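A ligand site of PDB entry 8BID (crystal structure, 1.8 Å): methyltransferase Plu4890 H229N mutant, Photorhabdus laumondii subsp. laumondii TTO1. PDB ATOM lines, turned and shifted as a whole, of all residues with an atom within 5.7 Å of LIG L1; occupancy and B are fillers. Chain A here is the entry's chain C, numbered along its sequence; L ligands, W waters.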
ATOM      1  N   PHE A 127       1.596  -5.227  23.344  1.00  0.00           N
ATOM      2  CA  PHE A 127       2.741  -6.137  23.650  1.00  0.00           C
ATOM      3  C   PHE A 127       3.915  -5.352  24.225  1.00  0.00           C
ATOM      4  O   PHE A 127       4.554  -5.845  25.172  1.00  0.00           O
ATOM      5  CB  PHE A 127       3.095  -6.996  22.424  1.00  0.00           C
ATOM      6  CG  PHE A 127       2.071  -8.072  22.164  1.00  0.00           C
ATOM      7  CD1 PHE A 127       1.827  -9.059  23.106  1.00  0.00           C
ATOM      8  CD2 PHE A 127       1.345  -8.091  20.989  1.00  0.00           C
ATOM      9  CE1 PHE A 127       0.879 -10.046  22.882  1.00  0.00           C
ATOM     10  CE2 PHE A 127       0.394  -9.072  20.759  1.00  0.00           C
ATOM     11  CZ  PHE A 127       0.165 -10.046  21.707  1.00  0.00           C
ATOM     12  N   LYS A 137       1.361  -9.641  31.410  1.00  0.00           N
ATOM     13  CA  LYS A 137       2.202 -10.545  30.582  1.00  0.00           C
ATOM     14  C   LYS A 137       2.052 -11.995  31.088  1.00  0.00           C
ATOM     15  O   LYS A 137       1.801 -12.866  30.249  1.00  0.00           O
ATOM     16  CB  LYS A 137       3.671 -10.126  30.562  1.00  0.00           C
ATOM     17  CG  LYS A 137       4.514 -10.963  29.617  1.00  0.00           C
ATOM     18  CD  LYS A 137       5.902 -10.431  29.347  1.00  0.00           C
ATOM     19  CE  LYS A 137       6.688 -11.367  28.458  1.00  0.00           C
ATOM     20  NZ  LYS A 137       6.036 -11.532  27.138  1.00  0.00           N
ATOM     21  N   PHE A 140      -1.622 -13.241  30.372  1.00  0.00           N
ATOM     22  CA  PHE A 140      -1.884 -13.338  28.915  1.00  0.00           C
ATOM     23  C   PHE A 140      -1.130 -14.540  28.342  1.00  0.00           C
ATOM     24  O   PHE A 140      -1.741 -15.348  27.586  1.00  0.00           O
ATOM     25  CB  PHE A 140      -1.517 -12.046  28.181  1.00  0.00           C
ATOM     26  CG  PHE A 140      -1.769 -12.143  26.704  1.00  0.00           C
ATOM     27  CD1 PHE A 140      -3.033 -11.921  26.187  1.00  0.00           C
ATOM     28  CD2 PHE A 140      -0.757 -12.514  25.828  1.00  0.00           C
ATOM     29  CE1 PHE A 140      -3.271 -12.052  24.824  1.00  0.00           C
ATOM     30  CE2 PHE A 140      -0.992 -12.616  24.467  1.00  0.00           C
ATOM     31  CZ  PHE A 140      -2.252 -12.412  23.975  1.00  0.00           C
ATOM     32  N   ASP A 141       0.157 -14.680  28.670  1.00  0.00           N
ATOM     33  CA  ASP A 141       1.013 -15.797  28.199  1.00  0.00           C
ATOM     34  C   ASP A 141       0.457 -17.126  28.733  1.00  0.00           C
ATOM     35  O   ASP A 141       0.496 -18.123  27.980  1.00  0.00           O
ATOM     36  CB  ASP A 141       2.492 -15.578  28.555  1.00  0.00           C
ATOM     37  CG  ASP A 141       3.224 -14.587  27.663  1.00  0.00           C
ATOM     38  OD1 ASP A 141       2.593 -14.067  26.711  1.00  0.00           O
ATOM     39  OD2 ASP A 141       4.408 -14.344  27.911  1.00  0.00           O
ATOM     40  N   MET A 144      -2.698 -18.119  26.705  1.00  0.00           N
ATOM     41  CA  MET A 144      -2.277 -18.599  25.362  1.00  0.00           C
ATOM     42  C   MET A 144      -1.706 -20.025  25.503  1.00  0.00           C
ATOM     43  O   MET A 144      -1.993 -20.879  24.653  1.00  0.00           O
ATOM     44  CB  MET A 144      -1.226 -17.679  24.722  1.00  0.00           C
ATOM     45  CG  MET A 144      -1.733 -16.274  24.393  1.00  0.00           C
ATOM     46  SD  MET A 144      -3.173 -16.220  23.287  1.00  0.00           S
ATOM     47  CE  MET A 144      -4.488 -15.951  24.461  1.00  0.00           C
ATOM     48  N   THR A 145      -0.962 -20.277  26.575  1.00  0.00           N
ATOM     49  CA  THR A 145      -0.392 -21.609  26.879  1.00  0.00           C
ATOM     50  C   THR A 145      -1.542 -22.622  27.016  1.00  0.00           C
ATOM     51  O   THR A 145      -1.422 -23.724  26.441  1.00  0.00           O
ATOM     52  CB  THR A 145       0.539 -21.524  28.085  1.00  0.00           C
ATOM     53  OG1 THR A 145       1.721 -20.888  27.614  1.00  0.00           O
ATOM     54  CG2 THR A 145       0.872 -22.869  28.714  1.00  0.00           C
ATOM     55  N   VAL A 147      -4.846 -22.526  25.853  1.00  0.00           N
ATOM     56  CA  VAL A 147      -5.626 -22.777  24.605  1.00  0.00           C
ATOM     57  C   VAL A 147      -4.741 -23.527  23.597  1.00  0.00           C
ATOM     58  O   VAL A 147      -5.294 -24.362  22.848  1.00  0.00           O
ATOM     59  CB  VAL A 147      -6.239 -21.491  24.006  1.00  0.00           C
ATOM     60  CG1 VAL A 147      -7.210 -20.855  24.983  1.00  0.00           C
ATOM     61  CG2 VAL A 147      -5.199 -20.477  23.549  1.00  0.00           C
ATOM     62  N   SER A 148      -3.430 -23.284  23.573  1.00  0.00           N
ATOM     63  CA  SER A 148      -2.445 -24.052  22.758  1.00  0.00           C
ATOM     64  C   SER A 148      -2.510 -25.525  23.179  1.00  0.00           C
ATOM     65  O   SER A 148      -2.616 -26.401  22.298  1.00  0.00           O
ATOM     66  CB  SER A 148      -1.041 -23.499  22.912  1.00  0.00           C
ATOM     67  OG  SER A 148      -0.932 -22.191  22.386  1.00  0.00           O
ATOM     68  N   ASP A 169       8.041 -22.320  15.307  1.00  0.00           N
ATOM     69  CA  ASP A 169       6.763 -21.687  15.726  1.00  0.00           C
ATOM     70  C   ASP A 169       7.013 -20.191  15.945  1.00  0.00           C
ATOM     71  O   ASP A 169       7.741 -19.837  16.900  1.00  0.00           O
ATOM     72  CB  ASP A 169       6.202 -22.392  16.960  1.00  0.00           C
ATOM     73  CG  ASP A 169       4.785 -21.971  17.339  1.00  0.00           C
ATOM     74  OD1 ASP A 169       4.107 -21.353  16.494  1.00  0.00           O
ATOM     75  OD2 ASP A 169       4.377 -22.282  18.480  1.00  0.00           O
ATOM     76  N   VAL A 170       6.448 -19.331  15.090  1.00  0.00           N
ATOM     77  CA  VAL A 170       6.699 -17.868  15.073  1.00  0.00           C
ATOM     78  C   VAL A 170       5.611 -17.180  15.924  1.00  0.00           C
ATOM     79  O   VAL A 170       4.426 -17.423  15.676  1.00  0.00           O
ATOM     80  CB  VAL A 170       6.758 -17.332  13.633  1.00  0.00           C
ATOM     81  CG1 VAL A 170       6.848 -15.815  13.577  1.00  0.00           C
ATOM     82  CG2 VAL A 170       7.916 -17.951  12.864  1.00  0.00           C
ATOM     83  N   GLY A 171       6.006 -16.367  16.901  1.00  0.00           N
ATOM     84  CA  GLY A 171       5.103 -15.827  17.927  1.00  0.00           C
ATOM     85  C   GLY A 171       4.600 -16.926  18.858  1.00  0.00           C
ATOM     86  O   GLY A 171       3.439 -16.852  19.304  1.00  0.00           O
ATOM     87  N   GLY A 172       5.454 -17.903  19.174  1.00  0.00           N
ATOM     88  CA  GLY A 172       5.060 -19.125  19.906  1.00  0.00           C
ATOM     89  C   GLY A 172       4.940 -18.934  21.412  1.00  0.00           C
ATOM     90  O   GLY A 172       4.651 -19.946  22.116  1.00  0.00           O
ATOM     91  N   GLY A 173       5.170 -17.720  21.921  1.00  0.00           N
ATOM     92  CA  GLY A 173       5.037 -17.387  23.359  1.00  0.00           C
ATOM     93  C   GLY A 173       5.927 -18.255  24.228  1.00  0.00           C
ATOM     94  O   GLY A 173       7.165 -18.248  24.005  1.00  0.00           O
ATOM     95  N   LEU A 193      10.235 -18.700  18.178  1.00  0.00           N
ATOM     96  CA  LEU A 193      10.587 -17.263  18.048  1.00  0.00           C
ATOM     97  C   LEU A 193       9.503 -16.419  18.741  1.00  0.00           C
ATOM     98  O   LEU A 193       8.299 -16.661  18.505  1.00  0.00           O
ATOM     99  CB  LEU A 193      10.708 -16.902  16.565  1.00  0.00           C
ATOM    100  CG  LEU A 193      11.245 -15.506  16.249  1.00  0.00           C
ATOM    101  CD1 LEU A 193      11.964 -15.492  14.916  1.00  0.00           C
ATOM    102  CD2 LEU A 193      10.143 -14.461  16.264  1.00  0.00           C
ATOM    103  N   ASP A 194       9.926 -15.459  19.556  1.00  0.00           N
ATOM    104  CA  ASP A 194       9.024 -14.468  20.192  1.00  0.00           C
ATOM    105  C   ASP A 194       9.923 -13.335  20.710  1.00  0.00           C
ATOM    106  O   ASP A 194      11.137 -13.368  20.401  1.00  0.00           O
ATOM    107  CB  ASP A 194       8.150 -15.114  21.269  1.00  0.00           C
ATOM    108  CG  ASP A 194       6.796 -14.452  21.483  1.00  0.00           C
ATOM    109  OD1 ASP A 194       6.797 -13.329  22.025  1.00  0.00           O
ATOM    110  OD2 ASP A 194       5.757 -15.060  21.105  1.00  0.00           O
ATOM    111  N   ARG A 195       9.327 -12.361  21.390  1.00  0.00           N
ATOM    112  CA  ARG A 195      10.034 -11.203  22.013  1.00  0.00           C
ATOM    113  C   ARG A 195      10.416 -11.611  23.429  1.00  0.00           C
ATOM    114  O   ARG A 195       9.524 -11.600  24.306  1.00  0.00           O
ATOM    115  CB  ARG A 195       9.151  -9.959  21.948  1.00  0.00           C
ATOM    116  CG  ARG A 195       8.804  -9.540  20.529  1.00  0.00           C
ATOM    117  CD  ARG A 195       7.923  -8.302  20.440  1.00  0.00           C
ATOM    118  NE  ARG A 195       8.557  -7.138  21.039  1.00  0.00           N
ATOM    119  CZ  ARG A 195       8.317  -6.682  22.268  1.00  0.00           C
ATOM    120  NH1 ARG A 195       7.446  -7.282  23.057  1.00  0.00           N
ATOM    121  NH2 ARG A 195       8.974  -5.622  22.700  1.00  0.00           N
ATOM    122  N   GLY A 210      13.319 -12.589  18.648  1.00  0.00           N
ATOM    123  CA  GLY A 210      13.184 -12.072  17.277  1.00  0.00           C
ATOM    124  C   GLY A 210      12.035 -11.082  17.166  1.00  0.00           C
ATOM    125  O   GLY A 210      11.393 -10.796  18.205  1.00  0.00           O
ATOM    126  N   ASN A 211      11.814 -10.613  15.942  1.00  0.00           N
ATOM    127  CA  ASN A 211      10.735  -9.652  15.583  1.00  0.00           C
ATOM    128  C   ASN A 211      10.237 -10.015  14.182  1.00  0.00           C
ATOM    129  O   ASN A 211      10.977  -9.786  13.224  1.00  0.00           O
ATOM    130  CB  ASN A 211      11.255  -8.212  15.638  1.00  0.00           C
ATOM    131  CG  ASN A 211      10.216  -7.195  15.214  1.00  0.00           C
ATOM    132  OD1 ASN A 211       9.063  -7.543  14.989  1.00  0.00           O
ATOM    133  ND2 ASN A 211      10.618  -5.948  15.095  1.00  0.00           N
ATOM    134  N   PHE A 212       9.028 -10.586  14.076  1.00  0.00           N
ATOM    135  CA  PHE A 212       8.471 -11.129  12.813  1.00  0.00           C
ATOM    136  C   PHE A 212       8.046  -9.990  11.884  1.00  0.00           C
ATOM    137  O   PHE A 212       7.710 -10.296  10.734  1.00  0.00           O
ATOM    138  CB  PHE A 212       7.347 -12.141  13.069  1.00  0.00           C
ATOM    139  CG  PHE A 212       6.215 -11.724  13.975  1.00  0.00           C
ATOM    140  CD1 PHE A 212       5.798 -12.558  15.002  1.00  0.00           C
ATOM    141  CD2 PHE A 212       5.526 -10.537  13.766  1.00  0.00           C
ATOM    142  CE1 PHE A 212       4.731 -12.209  15.829  1.00  0.00           C
ATOM    143  CE2 PHE A 212       4.466 -10.182  14.596  1.00  0.00           C
ATOM    144  CZ  PHE A 212       4.076 -11.011  15.616  1.00  0.00           C
ATOM    145  N   LEU A 213       8.066  -8.733  12.333  1.00  0.00           N
ATOM    146  CA  LEU A 213       7.799  -7.542  11.472  1.00  0.00           C
ATOM    147  C   LEU A 213       9.074  -7.178  10.681  1.00  0.00           C
ATOM    148  O   LEU A 213       8.938  -6.639   9.565  1.00  0.00           O
ATOM    149  CB  LEU A 213       7.357  -6.356  12.333  1.00  0.00           C
ATOM    150  CG  LEU A 213       6.094  -6.539  13.172  1.00  0.00           C
ATOM    151  CD1 LEU A 213       5.898  -5.356  14.092  1.00  0.00           C
ATOM    152  CD2 LEU A 213       4.871  -6.739  12.293  1.00  0.00           C
ATOM    153  N   LYS A 226       0.353 -19.263  14.815  1.00  0.00           N
ATOM    154  CA  LYS A 226      -0.946 -19.508  15.484  1.00  0.00           C
ATOM    155  C   LYS A 226      -1.372 -18.254  16.256  1.00  0.00           C
ATOM    156  O   LYS A 226      -0.587 -17.769  17.096  1.00  0.00           O
ATOM    157  CB  LYS A 226      -0.882 -20.718  16.435  1.00  0.00           C
ATOM    158  CG  LYS A 226      -2.241 -21.131  16.995  1.00  0.00           C
ATOM    159  CD  LYS A 226      -2.266 -22.501  17.652  1.00  0.00           C
ATOM    160  CE  LYS A 226      -1.540 -22.541  18.984  1.00  0.00           C
ATOM    161  NZ  LYS A 226      -2.215 -21.700  20.001  1.00  0.00           N
ATOM    162  N   ASN A 227      -2.584 -17.751  15.967  1.00  0.00           N
ATOM    163  CA  ASN A 227      -3.278 -16.673  16.738  1.00  0.00           C
ATOM    164  C   ASN A 227      -2.409 -15.415  16.816  1.00  0.00           C
ATOM    165  O   ASN A 227      -2.409 -14.754  17.882  1.00  0.00           O
ATOM    166  CB  ASN A 227      -3.676 -17.164  18.132  1.00  0.00           C
ATOM    167  CG  ASN A 227      -4.835 -18.132  18.097  1.00  0.00           C
ATOM    168  OD1 ASN A 227      -5.667 -18.080  17.204  1.00  0.00           O
ATOM    169  ND2 ASN A 227      -4.892 -19.005  19.086  1.00  0.00           N
ATOM    170  N   VAL A 228      -1.733 -15.061  15.728  1.00  0.00           N
ATOM    171  CA  VAL A 228      -0.870 -13.840  15.651  1.00  0.00           C
ATOM    172  C   VAL A 228      -1.591 -12.789  14.807  1.00  0.00           C
ATOM    173  O   VAL A 228      -1.662 -11.644  15.263  1.00  0.00           O
ATOM    174  CB  VAL A 228       0.530 -14.185  15.094  1.00  0.00           C
ATOM    175  CG1 VAL A 228       1.289 -12.929  14.685  1.00  0.00           C
ATOM    176  CG2 VAL A 228       1.346 -14.996  16.083  1.00  0.00           C
ATOM    177  N   ASN A 231      -4.045  -9.965  15.878  1.00  0.00           N
ATOM    178  CA  ASN A 231      -3.468  -8.837  16.657  1.00  0.00           C
ATOM    179  C   ASN A 231      -2.929  -7.744  15.718  1.00  0.00           C
ATOM    180  O   ASN A 231      -2.303  -6.811  16.257  1.00  0.00           O
ATOM    181  CB  ASN A 231      -2.339  -9.280  17.577  1.00  0.00           C
ATOM    182  CG  ASN A 231      -2.632 -10.542  18.360  1.00  0.00           C
ATOM    183  OD1 ASN A 231      -3.780 -10.850  18.669  1.00  0.00           O
ATOM    184  ND2 ASN A 231      -1.595 -11.284  18.674  1.00  0.00           N
ATOM    185  N   TRP A 232      -3.141  -7.830  14.397  1.00  0.00           N
ATOM    186  CA  TRP A 232      -2.461  -6.956  13.407  1.00  0.00           C
ATOM    187  C   TRP A 232      -3.432  -6.452  12.338  1.00  0.00           C
ATOM    188  O   TRP A 232      -4.425  -7.155  12.020  1.00  0.00           O
ATOM    189  CB  TRP A 232      -1.264  -7.695  12.787  1.00  0.00           C
ATOM    190  CG  TRP A 232      -0.239  -8.067  13.808  1.00  0.00           C
ATOM    191  CD1 TRP A 232      -0.084  -9.273  14.412  1.00  0.00           C
ATOM    192  CD2 TRP A 232       0.712  -7.187  14.439  1.00  0.00           C
ATOM    193  NE1 TRP A 232       0.906  -9.225  15.349  1.00  0.00           N
ATOM    194  CE2 TRP A 232       1.420  -7.954  15.384  1.00  0.00           C
ATOM    195  CE3 TRP A 232       1.042  -5.831  14.289  1.00  0.00           C
ATOM    196  CZ2 TRP A 232       2.432  -7.414  16.167  1.00  0.00           C
ATOM    197  CZ3 TRP A 232       2.053  -5.300  15.061  1.00  0.00           C
ATOM    198  CH2 TRP A 232       2.742  -6.081  15.982  1.00  0.00           C
HETATM  199  N1  LIG L   1       1.317 -18.482  19.166  1.00  0.00           N
HETATM  200  C1  LIG L   1       0.925 -18.456  20.604  1.00  0.00           C
HETATM  201  C2  LIG L   1       0.810 -17.023  21.132  1.00  0.00           C
HETATM  202  C3  LIG L   1      -0.070 -16.105  20.302  1.00  0.00           C
HETATM  203  S1  LIG L   1      -0.347 -14.508  21.103  1.00  0.00           S
HETATM  204  C4  LIG L   1      -0.417 -19.170  20.765  1.00  0.00           C
HETATM  205  O1  LIG L   1      -0.722 -19.675  21.838  1.00  0.00           O
HETATM  206  O2  LIG L   1      -1.184 -19.252  19.811  1.00  0.00           O
HETATM  207  C5  LIG L   1       0.698 -13.412  20.090  1.00  0.00           C
HETATM  208  C6  LIG L   1       2.187 -13.605  20.307  1.00  0.00           C
HETATM  209  O3  LIG L   1       2.930 -12.742  19.404  1.00  0.00           O
HETATM  210  C7  LIG L   1       2.682 -13.246  21.722  1.00  0.00           C
HETATM  211  O4  LIG L   1       3.393 -14.354  22.275  1.00  0.00           O
HETATM  212  C8  LIG L   1       3.586 -12.024  21.496  1.00  0.00           C
HETATM  213  O5  LIG L   1       4.668 -11.953  22.402  1.00  0.00           O
HETATM  214  C9  LIG L   1       4.077 -12.291  20.080  1.00  0.00           C
HETATM  215  N2  LIG L   1       4.609 -11.125  19.380  1.00  0.00           N
HETATM  216  C10 LIG L   1       4.059  -9.862  19.324  1.00  0.00           C
HETATM  217  N3  LIG L   1       4.750  -9.031  18.589  1.00  0.00           N
HETATM  218  C11 LIG L   1       5.820  -9.786  18.122  1.00  0.00           C
HETATM  219  C12 LIG L   1       6.895  -9.464  17.278  1.00  0.00           C
HETATM  220  N4  LIG L   1       7.084  -8.263  16.732  1.00  0.00           N
HETATM  221  N5  LIG L   1       7.781 -10.453  16.994  1.00  0.00           N
HETATM  222  C13 LIG L   1       7.587 -11.667  17.543  1.00  0.00           C
HETATM  223  N6  LIG L   1       6.614 -12.077  18.347  1.00  0.00           N
HETATM  224  C14 LIG L   1       5.748 -11.077  18.601  1.00  0.00           C
HETATM  225  O1  LG2 L   2      -7.168 -17.319  21.352  1.00  0.00           O
HETATM  226  C1  LG2 L   2      -7.467 -16.381  22.093  1.00  0.00           C
HETATM  227  C2  LG2 L   2      -8.442 -16.549  23.073  1.00  0.00           C
HETATM  228  C3  LG2 L   2      -9.085 -17.777  23.215  1.00  0.00           C
HETATM  229  C4  LG2 L   2     -10.065 -17.968  24.187  1.00  0.00           C
HETATM  230  C5  LG2 L   2     -10.415 -16.933  25.019  1.00  0.00           C
HETATM  231  C6  LG2 L   2      -9.778 -15.701  24.884  1.00  0.00           C
HETATM  232  O2  LG2 L   2     -10.104 -14.643  25.684  1.00  0.00           O
HETATM  233  C7  LG2 L   2      -8.792 -15.488  23.921  1.00  0.00           C
HETATM  234  C8  LG2 L   2      -8.160 -14.243  23.803  1.00  0.00           C
HETATM  235  O3  LG2 L   2      -8.475 -13.299  24.542  1.00  0.00           O
HETATM  236  C9  LG2 L   2      -7.166 -14.076  22.813  1.00  0.00           C
HETATM  237  C10 LG2 L   2      -6.823 -15.143  21.962  1.00  0.00           C
HETATM  238  C11 LG2 L   2      -5.838 -14.976  20.992  1.00  0.00           C
HETATM  239  C12 LG2 L   2      -5.178 -13.753  20.852  1.00  0.00           C
HETATM  240  O4  LG2 L   2      -4.207 -13.588  19.886  1.00  0.00           O
HETATM  241  C13 LG2 L   2      -5.526 -12.688  21.686  1.00  0.00           C
HETATM  242  C14 LG2 L   2      -6.509 -12.845  22.667  1.00  0.00           C
HETATM  243  O5  LG2 L   2      -6.927 -11.869  23.542  1.00  0.00           O
HETATM  244  C15 LG2 L   2      -6.189 -10.653  23.683  1.00  0.00           C
HETATM  245  O   HOH W   1       1.171 -10.920  17.824  1.00  0.00           O
HETATM  246  O   HOH W   2       5.726  -9.482  23.139  1.00  0.00           O
HETATM  247  O   HOH W   3       1.298 -19.933  23.500  1.00  0.00           O
HETATM  248  O   HOH W   4       5.110  -5.960  19.021  1.00  0.00           O
HETATM  249  O   HOH W   5       1.973 -21.195  19.033  1.00  0.00           O
HETATM  250  O   HOH W   6       2.071 -15.651  24.515  1.00  0.00           O
HETATM  251  O   HOH W   7       2.666 -19.174  16.655  1.00  0.00           O
HETATM  252  O   HOH W   8      -3.531 -18.670  21.508  1.00  0.00           O
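Water W2 bridges an oxygen (O5) of LIG L1 (2.8 Å) and the guanidinium group of Arg 195 (2.8 Å).
Water W5 bridges the side-chain carboxylate (OD2) of Asp 169 and a nitrogen (N1) of LIG L1.
Water W6 lies within hydrogen-bond range of OD1 of Asp 141 and O4 of LIG L1.
Water W7 lies within hydrogen-bond range of OD1 of Asp 169, O of Val 170, N1 of LIG L1 and N of Lys 226.
Water W8 lies within hydrogen-bond range of the side-chain amide nitrogen (ND2) of Asn 227 (2.8 Å), an oxygen (O2) of LIG L1 (3.0 Å) and the side-chain sulfur (SD) of Met 144 (3.0 Å).
Water W1 lies within hydrogen-bond range of ND2 of Asn 231 (2.9 Å), O3 of LIG L1 (3.0 Å) and NE1 of Trp 232 (3.0 Å).
O1 of LIG L1 sits close to O of Met 144, 3.3 Å away.
Merely in contact with LIG L1: Phe 127, Phe 140, Gly 172, Gly 173, Leu 193, Arg 195, Gly 210, Asn 227, Asn 231 and Trp 232.
Hydrophobic or aromatic side chains that line LIG L1: Phe 127, Phe 140, Met 144, Leu 193, Phe 212 and Trp 232.
17 residues have an atom within 4 Å of LIG L1: Phe 127, Phe 140, Met 144, Ser 148, Gly 171, Gly 172, Gly 173, Leu 193, Asp 194, Arg 195, Gly 210, Asn 211, Phe 212, Lys 226, Asn 227, Asn 231 and Trp 232.
N of Phe 212 sits at hydrogen-bond distance from N5 of LIG L1 (3.2 Å).
A nitrogen (N1) of LIG L1 lies within hydrogen-bond range of the backbone carbonyl oxygen of Gly 171, at 2.7 Å.
The side-chain amide oxygen (OD1) of Asn 211 is in hydrogen-bond range of a nitrogen (N4) of LIG L1 (2.7 Å).
O2 of LIG L1 is in salt-bridge range of NZ of Lys 226, at 2.7 Å.
The backbone carbonyl oxygen (O) of Lys 226 lies within hydrogen-bond range of a nitrogen (N1) of LIG L1, at 2.9 Å.
O5 of LIG L1 is in hydrogen-bond range of OD1 of Asp 194, at 2.6 Å.
O4 of LG2 L2 lies within hydrogen-bond range of O of Asn 227, 2.9 Å away.
OD1 of Asn 231 is in hydrogen-bond range of O4 of LG2 L2.
The side-chain hydroxyl of Ser 148 sits at hydrogen-bond distance from an oxygen (O1) of LIG L1.
The backbone carbonyl oxygen (O) of Val 228 lies close to the side-chain amide nitrogen (ND2) of Asn 231, at 3.4 Å.
The backbone carbonyl oxygen (O) of Leu 193 lies within hydrogen-bond range of the backbone NH (N) of Gly 171.
The backbone NH (N) of Gly 173 sits at hydrogen-bond distance from the side-chain carboxylate (OD2) of Asp 194 (2.8 Å).
The side-chain hydroxyl (OG) of Ser 148 is in hydrogen-bond range of the side-chain amino group (NZ) of Lys 226 (2.8 Å).
The backbone NH of Leu 213 is in hydrogen-bond range of the side-chain amide oxygen of Asn 211 (3.1 Å).
N of Gly 172 lies within hydrogen-bond range of OD2 of Asp 194 (3.5 Å).
The backbone NH (N) of Gly 172 sits at hydrogen-bond distance from the backbone carbonyl oxygen (O) of Leu 193, 3.2 Å away.
The side-chain hydroxyl (OG) of Ser 148 lies within hydrogen-bond range of the backbone carbonyl oxygen (O) of Met 144.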
